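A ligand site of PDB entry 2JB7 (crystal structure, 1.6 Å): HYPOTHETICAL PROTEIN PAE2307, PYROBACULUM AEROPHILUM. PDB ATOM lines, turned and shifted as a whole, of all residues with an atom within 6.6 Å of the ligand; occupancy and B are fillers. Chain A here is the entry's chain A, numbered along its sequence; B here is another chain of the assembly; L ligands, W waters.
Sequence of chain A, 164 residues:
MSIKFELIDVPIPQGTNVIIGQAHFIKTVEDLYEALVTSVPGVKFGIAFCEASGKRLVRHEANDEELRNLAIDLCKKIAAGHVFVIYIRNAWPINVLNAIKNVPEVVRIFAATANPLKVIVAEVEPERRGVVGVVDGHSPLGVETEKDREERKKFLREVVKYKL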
ATOM      1  N   THR A  16     -14.579  12.218 -20.436  1.00  0.00           N
ATOM      2  CA  THR A  16     -15.314  13.106 -19.521  1.00  0.00           C
ATOM      3  C   THR A  16     -14.362  14.123 -18.876  1.00  0.00           C
ATOM      4  O   THR A  16     -13.122  13.922 -18.789  1.00  0.00           O
ATOM      5  CB  THR A  16     -16.072  12.328 -18.423  1.00  0.00           C
ATOM      6  OG1 THR A  16     -15.168  11.806 -17.435  1.00  0.00           O
ATOM      7  CG2 THR A  16     -16.931  11.193 -19.019  1.00  0.00           C
ATOM      8  N   ASN A  17     -15.002  15.200 -18.381  1.00  0.00           N
ATOM      9  CA  ASN A  17     -14.395  16.126 -17.467  1.00  0.00           C
ATOM     10  C   ASN A  17     -15.268  16.282 -16.242  1.00  0.00           C
ATOM     11  O   ASN A  17     -16.476  16.065 -16.297  1.00  0.00           O
ATOM     12  CB  ASN A  17     -14.142  17.479 -18.098  1.00  0.00           C
ATOM     13  CG  ASN A  17     -12.980  17.474 -19.026  1.00  0.00           C
ATOM     14  OD1 ASN A  17     -13.090  17.038 -20.195  1.00  0.00           O
ATOM     15  ND2 ASN A  17     -11.842  17.929 -18.537  1.00  0.00           N
ATOM     16  N   VAL A  18     -14.656  16.566 -15.105  1.00  0.00           N
ATOM     17  CA  VAL A  18     -15.423  16.797 -13.891  1.00  0.00           C
ATOM     18  C   VAL A  18     -15.244  18.251 -13.432  1.00  0.00           C
ATOM     19  O   VAL A  18     -14.166  18.814 -13.605  1.00  0.00           O
ATOM     20  CB  VAL A  18     -15.032  15.807 -12.777  1.00  0.00           C
ATOM     21  CG1 VAL A  18     -13.659  16.168 -12.143  1.00  0.00           C
ATOM     22  CG2 VAL A  18     -16.143  15.722 -11.713  1.00  0.00           C
ATOM     23  N   TRP A  92     -15.975  20.954 -23.154  1.00  0.00           N
ATOM     24  CA  TRP A  92     -14.876  21.175 -22.223  1.00  0.00           C
ATOM     25  C   TRP A  92     -15.270  22.101 -21.088  1.00  0.00           C
ATOM     26  O   TRP A  92     -16.115  22.981 -21.272  1.00  0.00           O
ATOM     27  CB  TRP A  92     -13.729  21.854 -22.944  1.00  0.00           C
ATOM     28  CG  TRP A  92     -13.167  21.054 -24.079  1.00  0.00           C
ATOM     29  CD1 TRP A  92     -13.376  21.293 -25.424  1.00  0.00           C
ATOM     30  CD2 TRP A  92     -12.320  19.919 -23.988  1.00  0.00           C
ATOM     31  NE1 TRP A  92     -12.669  20.362 -26.167  1.00  0.00           N
ATOM     32  CE2 TRP A  92     -12.018  19.515 -25.316  1.00  0.00           C
ATOM     33  CE3 TRP A  92     -11.770  19.208 -22.929  1.00  0.00           C
ATOM     34  CZ2 TRP A  92     -11.181  18.440 -25.584  1.00  0.00           C
ATOM     35  CZ3 TRP A  92     -10.903  18.142 -23.201  1.00  0.00           C
ATOM     36  CH2 TRP A  92     -10.656  17.765 -24.534  1.00  0.00           C
ATOM     37  N   PRO A  93     -14.604  21.968 -19.914  1.00  0.00           N
ATOM     38  CA  PRO A  93     -14.885  22.957 -18.879  1.00  0.00           C
ATOM     39  C   PRO A  93     -14.769  24.411 -19.316  1.00  0.00           C
ATOM     40  O   PRO A  93     -15.584  25.209 -18.898  1.00  0.00           O
ATOM     41  CB  PRO A  93     -13.879  22.608 -17.764  1.00  0.00           C
ATOM     42  CG  PRO A  93     -13.714  21.137 -17.912  1.00  0.00           C
ATOM     43  CD  PRO A  93     -13.723  20.900 -19.417  1.00  0.00           C
ATOM     44  N   ILE A  94     -13.837  24.762 -20.191  1.00  0.00           N
ATOM     45  CA  ILE A  94     -13.733  26.180 -20.583  1.00  0.00           C
ATOM     46  C   ILE A  94     -14.993  26.645 -21.343  1.00  0.00           C
ATOM     47  O   ILE A  94     -15.245  27.848 -21.452  1.00  0.00           O
ATOM     48  CB  ILE A  94     -12.476  26.499 -21.461  1.00  0.00           C
ATOM     49  CG1 ILE A  94     -12.436  25.663 -22.741  1.00  0.00           C
ATOM     50  CG2 ILE A  94     -11.163  26.368 -20.620  1.00  0.00           C
ATOM     51  CD1 ILE A  94     -11.318  26.147 -23.712  1.00  0.00           C
ATOM     52  N   ASN A  95     -15.745  25.693 -21.894  1.00  0.00           N
ATOM     53  CA  ASN A  95     -16.963  26.025 -22.590  1.00  0.00           C
ATOM     54  C   ASN A  95     -18.087  26.419 -21.660  1.00  0.00           C
ATOM     55  O   ASN A  95     -19.035  27.071 -22.108  1.00  0.00           O
ATOM     56  CB  ASN A  95     -17.501  24.857 -23.438  1.00  0.00           C
ATOM     57  CG  ASN A  95     -16.530  24.365 -24.521  1.00  0.00           C
ATOM     58  OD1 ASN A  95     -15.710  25.118 -25.114  1.00  0.00           O
ATOM     59  ND2 ASN A  95     -16.637  23.094 -24.793  1.00  0.00           N
ATOM     60  N   ALA A 112     -11.687  21.876 -11.996  1.00  0.00           N
ATOM     61  CA  ALA A 112     -12.265  21.574 -13.300  1.00  0.00           C
ATOM     62  C   ALA A 112     -11.169  20.816 -14.071  1.00  0.00           C
ATOM     63  O   ALA A 112     -10.128  21.395 -14.359  1.00  0.00           O
ATOM     64  CB  ALA A 112     -12.686  22.813 -14.006  1.00  0.00           C
ATOM     65  N   THR A 113     -11.378  19.517 -14.352  1.00  0.00           N
ATOM     66  CA  THR A 113     -10.256  18.695 -14.757  1.00  0.00           C
ATOM     67  C   THR A 113     -10.673  17.340 -15.276  1.00  0.00           C
ATOM     68  O   THR A 113     -11.794  16.879 -14.977  1.00  0.00           O
ATOM     69  CB  THR A 113      -9.292  18.481 -13.572  1.00  0.00           C
ATOM     70  OG1 THR A 113      -7.998  18.027 -14.045  1.00  0.00           O
ATOM     71  CG2 THR A 113      -9.835  17.489 -12.594  1.00  0.00           C
ATOM     72  N   ALA A 114      -9.790  16.700 -16.043  1.00  0.00           N
ATOM     73  CA  ALA A 114      -9.934  15.304 -16.422  1.00  0.00           C
ATOM     74  C   ALA A 114      -8.727  14.485 -15.934  1.00  0.00           C
ATOM     75  O   ALA A 114      -8.628  13.318 -16.249  1.00  0.00           O
ATOM     76  CB  ALA A 114     -10.116  15.160 -17.946  1.00  0.00           C
ATOM     77  N   ASN A 115      -7.860  15.097 -15.129  1.00  0.00           N
ATOM     78  CA  ASN A 115      -6.725  14.423 -14.480  1.00  0.00           C
ATOM     79  C   ASN A 115      -7.129  13.517 -13.340  1.00  0.00           C
ATOM     80  O   ASN A 115      -8.206  13.691 -12.762  1.00  0.00           O
ATOM     81  CB  ASN A 115      -5.766  15.446 -13.876  1.00  0.00           C
ATOM     82  CG  ASN A 115      -5.063  16.254 -14.915  1.00  0.00           C
ATOM     83  OD1 ASN A 115      -4.811  15.803 -16.027  1.00  0.00           O
ATOM     84  ND2 ASN A 115      -4.656  17.425 -14.533  1.00  0.00           N
ATOM     85  N   ASP A 136      -5.251  17.908  -7.887  1.00  0.00           N
ATOM     86  CA  ASP A 136      -5.550  17.869  -9.293  1.00  0.00           C
ATOM     87  C   ASP A 136      -4.275  17.436 -10.040  1.00  0.00           C
ATOM     88  O   ASP A 136      -3.335  18.220 -10.178  1.00  0.00           O
ATOM     89  CB  ASP A 136      -6.111  19.232  -9.767  1.00  0.00           C
ATOM     90  CG  ASP A 136      -6.510  19.268 -11.221  1.00  0.00           C
ATOM     91  OD1 ASP A 136      -6.239  18.318 -11.995  1.00  0.00           O
ATOM     92  OD2 ASP A 136      -7.152  20.308 -11.611  1.00  0.00           O
ATOM     93  N   PHE A 155       0.724  24.024 -30.552  1.00  0.00           N
ATOM     94  CA  PHE A 155      -0.414  23.162 -30.220  1.00  0.00           C
ATOM     95  C   PHE A 155      -1.681  23.991 -30.246  1.00  0.00           C
ATOM     96  O   PHE A 155      -2.692  23.613 -30.855  1.00  0.00           O
ATOM     97  CB  PHE A 155      -0.218  22.552 -28.845  1.00  0.00           C
ATOM     98  CG  PHE A 155      -1.408  21.842 -28.332  1.00  0.00           C
ATOM     99  CD1 PHE A 155      -1.817  20.652 -28.907  1.00  0.00           C
ATOM    100  CD2 PHE A 155      -2.141  22.358 -27.287  1.00  0.00           C
ATOM    101  CE1 PHE A 155      -2.937  19.998 -28.455  1.00  0.00           C
ATOM    102  CE2 PHE A 155      -3.276  21.691 -26.826  1.00  0.00           C
ATOM    103  CZ  PHE A 155      -3.662  20.520 -27.410  1.00  0.00           C
ATOM    104  N   VAL A 160      -5.542  22.607 -31.733  1.00  0.00           N
ATOM    105  CA  VAL A 160      -6.867  22.967 -31.161  1.00  0.00           C
ATOM    106  C   VAL A 160      -7.387  24.303 -31.691  1.00  0.00           C
ATOM    107  O   VAL A 160      -8.586  24.592 -31.597  1.00  0.00           O
ATOM    108  CB  VAL A 160      -6.884  22.905 -29.609  1.00  0.00           C
ATOM    109  CG1 VAL A 160      -6.819  21.453 -29.120  1.00  0.00           C
ATOM    110  CG2 VAL A 160      -5.774  23.707 -28.980  1.00  0.00           C
ATOM    111  N   TYR A 162      -7.207  27.364 -30.830  1.00  0.00           N
ATOM    112  CA  TYR A 162      -7.759  28.340 -29.885  1.00  0.00           C
ATOM    113  C   TYR A 162      -7.090  29.702 -29.932  1.00  0.00           C
ATOM    114  O   TYR A 162      -7.601  30.680 -29.338  1.00  0.00           O
ATOM    115  CB  TYR A 162      -7.682  27.800 -28.442  1.00  0.00           C
ATOM    116  CG  TYR A 162      -8.601  26.636 -28.116  1.00  0.00           C
ATOM    117  CD1 TYR A 162      -9.815  26.448 -28.758  1.00  0.00           C
ATOM    118  CD2 TYR A 162      -8.244  25.744 -27.129  1.00  0.00           C
ATOM    119  CE1 TYR A 162     -10.647  25.387 -28.382  1.00  0.00           C
ATOM    120  CE2 TYR A 162      -9.067  24.669 -26.768  1.00  0.00           C
ATOM    121  CZ  TYR A 162     -10.273  24.507 -27.395  1.00  0.00           C
ATOM    122  OH  TYR A 162     -11.074  23.435 -27.037  1.00  0.00           O
ATOM    123  N   HIS B  24      -6.663  25.139 -15.017  1.00  0.00           N
ATOM    124  CA  HIS B  24      -6.567  23.862 -15.733  1.00  0.00           C
ATOM    125  C   HIS B  24      -6.299  24.214 -17.199  1.00  0.00           C
ATOM    126  O   HIS B  24      -6.691  25.275 -17.670  1.00  0.00           O
ATOM    127  CB  HIS B  24      -7.837  23.011 -15.573  1.00  0.00           C
ATOM    128  CG  HIS B  24      -8.969  23.443 -16.458  1.00  0.00           C
ATOM    129  ND1 HIS B  24      -9.585  24.671 -16.339  1.00  0.00           N
ATOM    130  CD2 HIS B  24      -9.604  22.789 -17.449  1.00  0.00           C
ATOM    131  CE1 HIS B  24     -10.546  24.763 -17.252  1.00  0.00           C
ATOM    132  NE2 HIS B  24     -10.572  23.630 -17.933  1.00  0.00           N
ATOM    133  N   PHE B  25      -5.616  23.318 -17.909  1.00  0.00           N
ATOM    134  CA  PHE B  25      -5.397  23.405 -19.356  1.00  0.00           C
ATOM    135  C   PHE B  25      -4.255  24.368 -19.685  1.00  0.00           C
ATOM    136  O   PHE B  25      -4.121  25.429 -19.124  1.00  0.00           O
ATOM    137  CB  PHE B  25      -6.685  23.786 -20.111  1.00  0.00           C
ATOM    138  CG  PHE B  25      -6.583  23.705 -21.629  1.00  0.00           C
ATOM    139  CD1 PHE B  25      -5.995  22.614 -22.253  1.00  0.00           C
ATOM    140  CD2 PHE B  25      -7.098  24.728 -22.401  1.00  0.00           C
ATOM    141  CE1 PHE B  25      -5.907  22.523 -23.594  1.00  0.00           C
ATOM    142  CE2 PHE B  25      -6.999  24.654 -23.802  1.00  0.00           C
ATOM    143  CZ  PHE B  25      -6.396  23.559 -24.388  1.00  0.00           C
ATOM    144  N   ILE B  26      -3.426  23.945 -20.632  1.00  0.00           N
ATOM    145  CA  ILE B  26      -2.225  24.697 -20.960  1.00  0.00           C
ATOM    146  C   ILE B  26      -2.465  26.140 -21.368  1.00  0.00           C
ATOM    147  O   ILE B  26      -1.595  27.018 -21.158  1.00  0.00           O
ATOM    148  CB  ILE B  26      -1.430  23.911 -22.049  1.00  0.00           C
ATOM    149  CG1 ILE B  26       0.040  24.348 -22.009  1.00  0.00           C
ATOM    150  CG2 ILE B  26      -2.104  24.032 -23.413  1.00  0.00           C
ATOM    151  CD1 ILE B  26       0.985  23.154 -22.022  1.00  0.00           C
ATOM    152  N   GLU B  51       1.407  22.615 -15.101  1.00  0.00           N
ATOM    153  CA  GLU B  51       0.826  21.547 -15.887  1.00  0.00           C
ATOM    154  C   GLU B  51       0.888  20.288 -15.029  1.00  0.00           C
ATOM    155  O   GLU B  51       1.928  19.982 -14.462  1.00  0.00           O
ATOM    156  CB  GLU B  51       1.634  21.360 -17.181  1.00  0.00           C
ATOM    157  CG  GLU B  51       1.210  20.187 -17.978  1.00  0.00           C
ATOM    158  CD  GLU B  51       2.100  19.953 -19.162  1.00  0.00           C
ATOM    159  OE1 GLU B  51       3.318  20.229 -19.042  1.00  0.00           O
ATOM    160  OE2 GLU B  51       1.569  19.499 -20.197  1.00  0.00           O
ATOM    161  N   ALA B  52      -0.235  19.575 -14.945  1.00  0.00           N
ATOM    162  CA  ALA B  52      -0.395  18.520 -13.947  1.00  0.00           C
ATOM    163  C   ALA B  52      -0.486  17.111 -14.546  1.00  0.00           C
ATOM    164  O   ALA B  52      -0.667  16.169 -13.799  1.00  0.00           O
ATOM    165  CB  ALA B  52      -1.599  18.798 -13.093  1.00  0.00           C
ATOM    166  N   SER B  53      -0.315  17.006 -15.864  1.00  0.00           N
ATOM    167  CA  SER B  53      -0.240  15.741 -16.584  1.00  0.00           C
ATOM    168  C   SER B  53       0.744  15.902 -17.712  1.00  0.00           C
ATOM    169  O   SER B  53       1.339  16.979 -17.875  1.00  0.00           O
ATOM    170  CB  SER B  53      -1.606  15.405 -17.171  1.00  0.00           C
ATOM    171  OG  SER B  53      -1.994  16.450 -18.044  1.00  0.00           O
ATOM    172  N   GLY B  54       0.930  14.829 -18.479  1.00  0.00           N
ATOM    173  CA  GLY B  54       1.861  14.838 -19.633  1.00  0.00           C
ATOM    174  C   GLY B  54       3.260  15.087 -19.166  1.00  0.00           C
ATOM    175  O   GLY B  54       3.734  14.449 -18.244  1.00  0.00           O
ATOM    176  N   HIS B  82      -1.871  22.155 -11.310  1.00  0.00           N
ATOM    177  CA  HIS B  82      -2.788  23.188 -11.778  1.00  0.00           C
ATOM    178  C   HIS B  82      -2.814  24.489 -10.995  1.00  0.00           C
ATOM    179  O   HIS B  82      -3.637  25.352 -11.302  1.00  0.00           O
ATOM    180  CB  HIS B  82      -4.191  22.613 -12.009  1.00  0.00           C
ATOM    181  CG  HIS B  82      -4.313  21.872 -13.300  1.00  0.00           C
ATOM    182  ND1 HIS B  82      -5.393  21.070 -13.589  1.00  0.00           N
ATOM    183  CD2 HIS B  82      -3.516  21.830 -14.390  1.00  0.00           C
ATOM    184  CE1 HIS B  82      -5.251  20.566 -14.798  1.00  0.00           C
ATOM    185  NE2 HIS B  82      -4.128  21.019 -15.318  1.00  0.00           N
HETATM  186  P1  LIG L   1      -4.390  17.238 -20.726  1.00  0.00           P
HETATM  187  O1  LIG L   1      -5.313  16.773 -21.840  1.00  0.00           O
HETATM  188  O2  LIG L   1      -3.038  17.621 -21.251  1.00  0.00           O
HETATM  189  O3  LIG L   1      -4.346  16.298 -19.528  1.00  0.00           O
HETATM  190  O4  LIG L   1      -5.011  18.694 -20.270  1.00  0.00           O
HETATM  191  C1  LIG L   1      -5.334  19.148 -18.947  1.00  0.00           C
HETATM  192  C2  LIG L   1      -6.813  19.528 -18.824  1.00  0.00           C
HETATM  193  O5  LIG L   1      -7.196  20.565 -19.740  1.00  0.00           O
HETATM  194  C3  LIG L   1      -7.712  18.335 -19.123  1.00  0.00           C
HETATM  195  O6  LIG L   1      -7.888  17.485 -17.990  1.00  0.00           O
HETATM  196  C4  LIG L   1      -8.987  19.043 -19.532  1.00  0.00           C
HETATM  197  O7  LIG L   1      -9.769  19.384 -18.373  1.00  0.00           O
HETATM  198  C5  LIG L   1      -8.500  20.300 -20.228  1.00  0.00           C
HETATM  199  N1  LIG L   1      -8.351  20.153 -21.687  1.00  0.00           N
HETATM  200  C6  LIG L   1      -7.538  19.281 -22.320  1.00  0.00           C
HETATM  201  N2  LIG L   1      -7.615  19.433 -23.668  1.00  0.00           N
HETATM  202  C7  LIG L   1      -8.520  20.418 -23.909  1.00  0.00           C
HETATM  203  C8  LIG L   1      -9.064  21.099 -25.080  1.00  0.00           C
HETATM  204  N3  LIG L   1      -8.722  20.743 -26.362  1.00  0.00           N
HETATM  205  N4  LIG L   1      -9.948  22.100 -24.905  1.00  0.00           N
HETATM  206  C9  LIG L   1     -10.336  22.486 -23.690  1.00  0.00           C
HETATM  207  N5  LIG L   1      -9.871  21.919 -22.562  1.00  0.00           N
HETATM  208  C10 LIG L   1      -8.975  20.905 -22.608  1.00  0.00           C
HETATM  209  O   HOH W   1     -10.242  20.517 -28.847  1.00  0.00           O
HETATM  210  O   HOH W   2      -3.223  21.217 -21.169  1.00  0.00           O
HETATM  211  O   HOH W   3      -8.607  15.698 -21.603  1.00  0.00           O
HETATM  212  O   HOH W   4     -11.544  22.954 -20.413  1.00  0.00           O
HETATM  213  O   HOH W   5      -3.347  13.786 -20.082  1.00  0.00           O
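The side-chain amide nitrogen (ND2) of Asn 95 lies close to the backbone NH (N) of Trp 92.
OD1 of Asp 136 sits at hydrogen-bond distance from OG1 of Thr 113 (2.7 Å).
The backbone carbonyl oxygen (O) of Thr 113 lies within hydrogen-bond range of the backbone NH (N) of Val 18, 2.9 Å away.
The side-chain amide nitrogen (ND2) of Asn 17 sits close to the backbone NH (N) of Ala 114, at 3.5 Å.
N of Val 160 lies within hydrogen-bond range of O of Phe 155 (3.1 Å).
The side-chain amide nitrogen (ND2) of Asn 115 is in hydrogen-bond range of the side-chain carboxylate (OD1) of Asp 136 (3.1 Å).
N of Asn 115 sits at hydrogen-bond distance from OG1 of Thr 113 (3.1 Å).
Residues that only touch the ligand: Ile 94 (3.8 Å), Thr 113 (3.7 Å), Asn 115 (3.6 Å), Val 160 (3.4 Å), His 24 of chain B (3.5 Å) and Phe 25 of chain B (3.3 Å).
Hydrophobic or aromatic side chains within 4 Å of the ligand: Trp 92, Ile 94, Ala 114, Val 160, Tyr 162, His 24 of chain B and Phe 25 of chain B.
Within 4 Å of the ligand: Asn 17, Trp 92, Ile 94, Thr 113, Ala 114, Asn 115, Val 160, Tyr 162, His 24 of chain B, Phe 25 of chain B and Ser 53 of chain B.
An oxygen (O3) of the ligand is in hydrogen-bond range of the side-chain hydroxyl (OG) of Ser 53 of chain B (2.8 Å).
The backbone NH (N) of Ala 114 is in hydrogen-bond range of an oxygen (O6) of the ligand, at 2.8 Å.
An oxygen (O7) of the ligand sits at hydrogen-bond distance from the side-chain amide nitrogen (ND2) of Asn 17 (2.5 Å).
The side-chain hydroxyl (OH) of Tyr 162 lies within hydrogen-bond range of a nitrogen (N4) of the ligand, 2.8 Å away.
N4 of the ligand sits close to NE1 of Trp 92, 3.5 Å away.
Water W4 lies within hydrogen-bond range of NE2 of His 24 of chain B, N5 of the ligand and N of Ile 94.
Water W2 bridges the backbone NH of Ile 26 of chain B (2.8 Å) and an oxygen (O4) of the ligand (3.2 Å).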
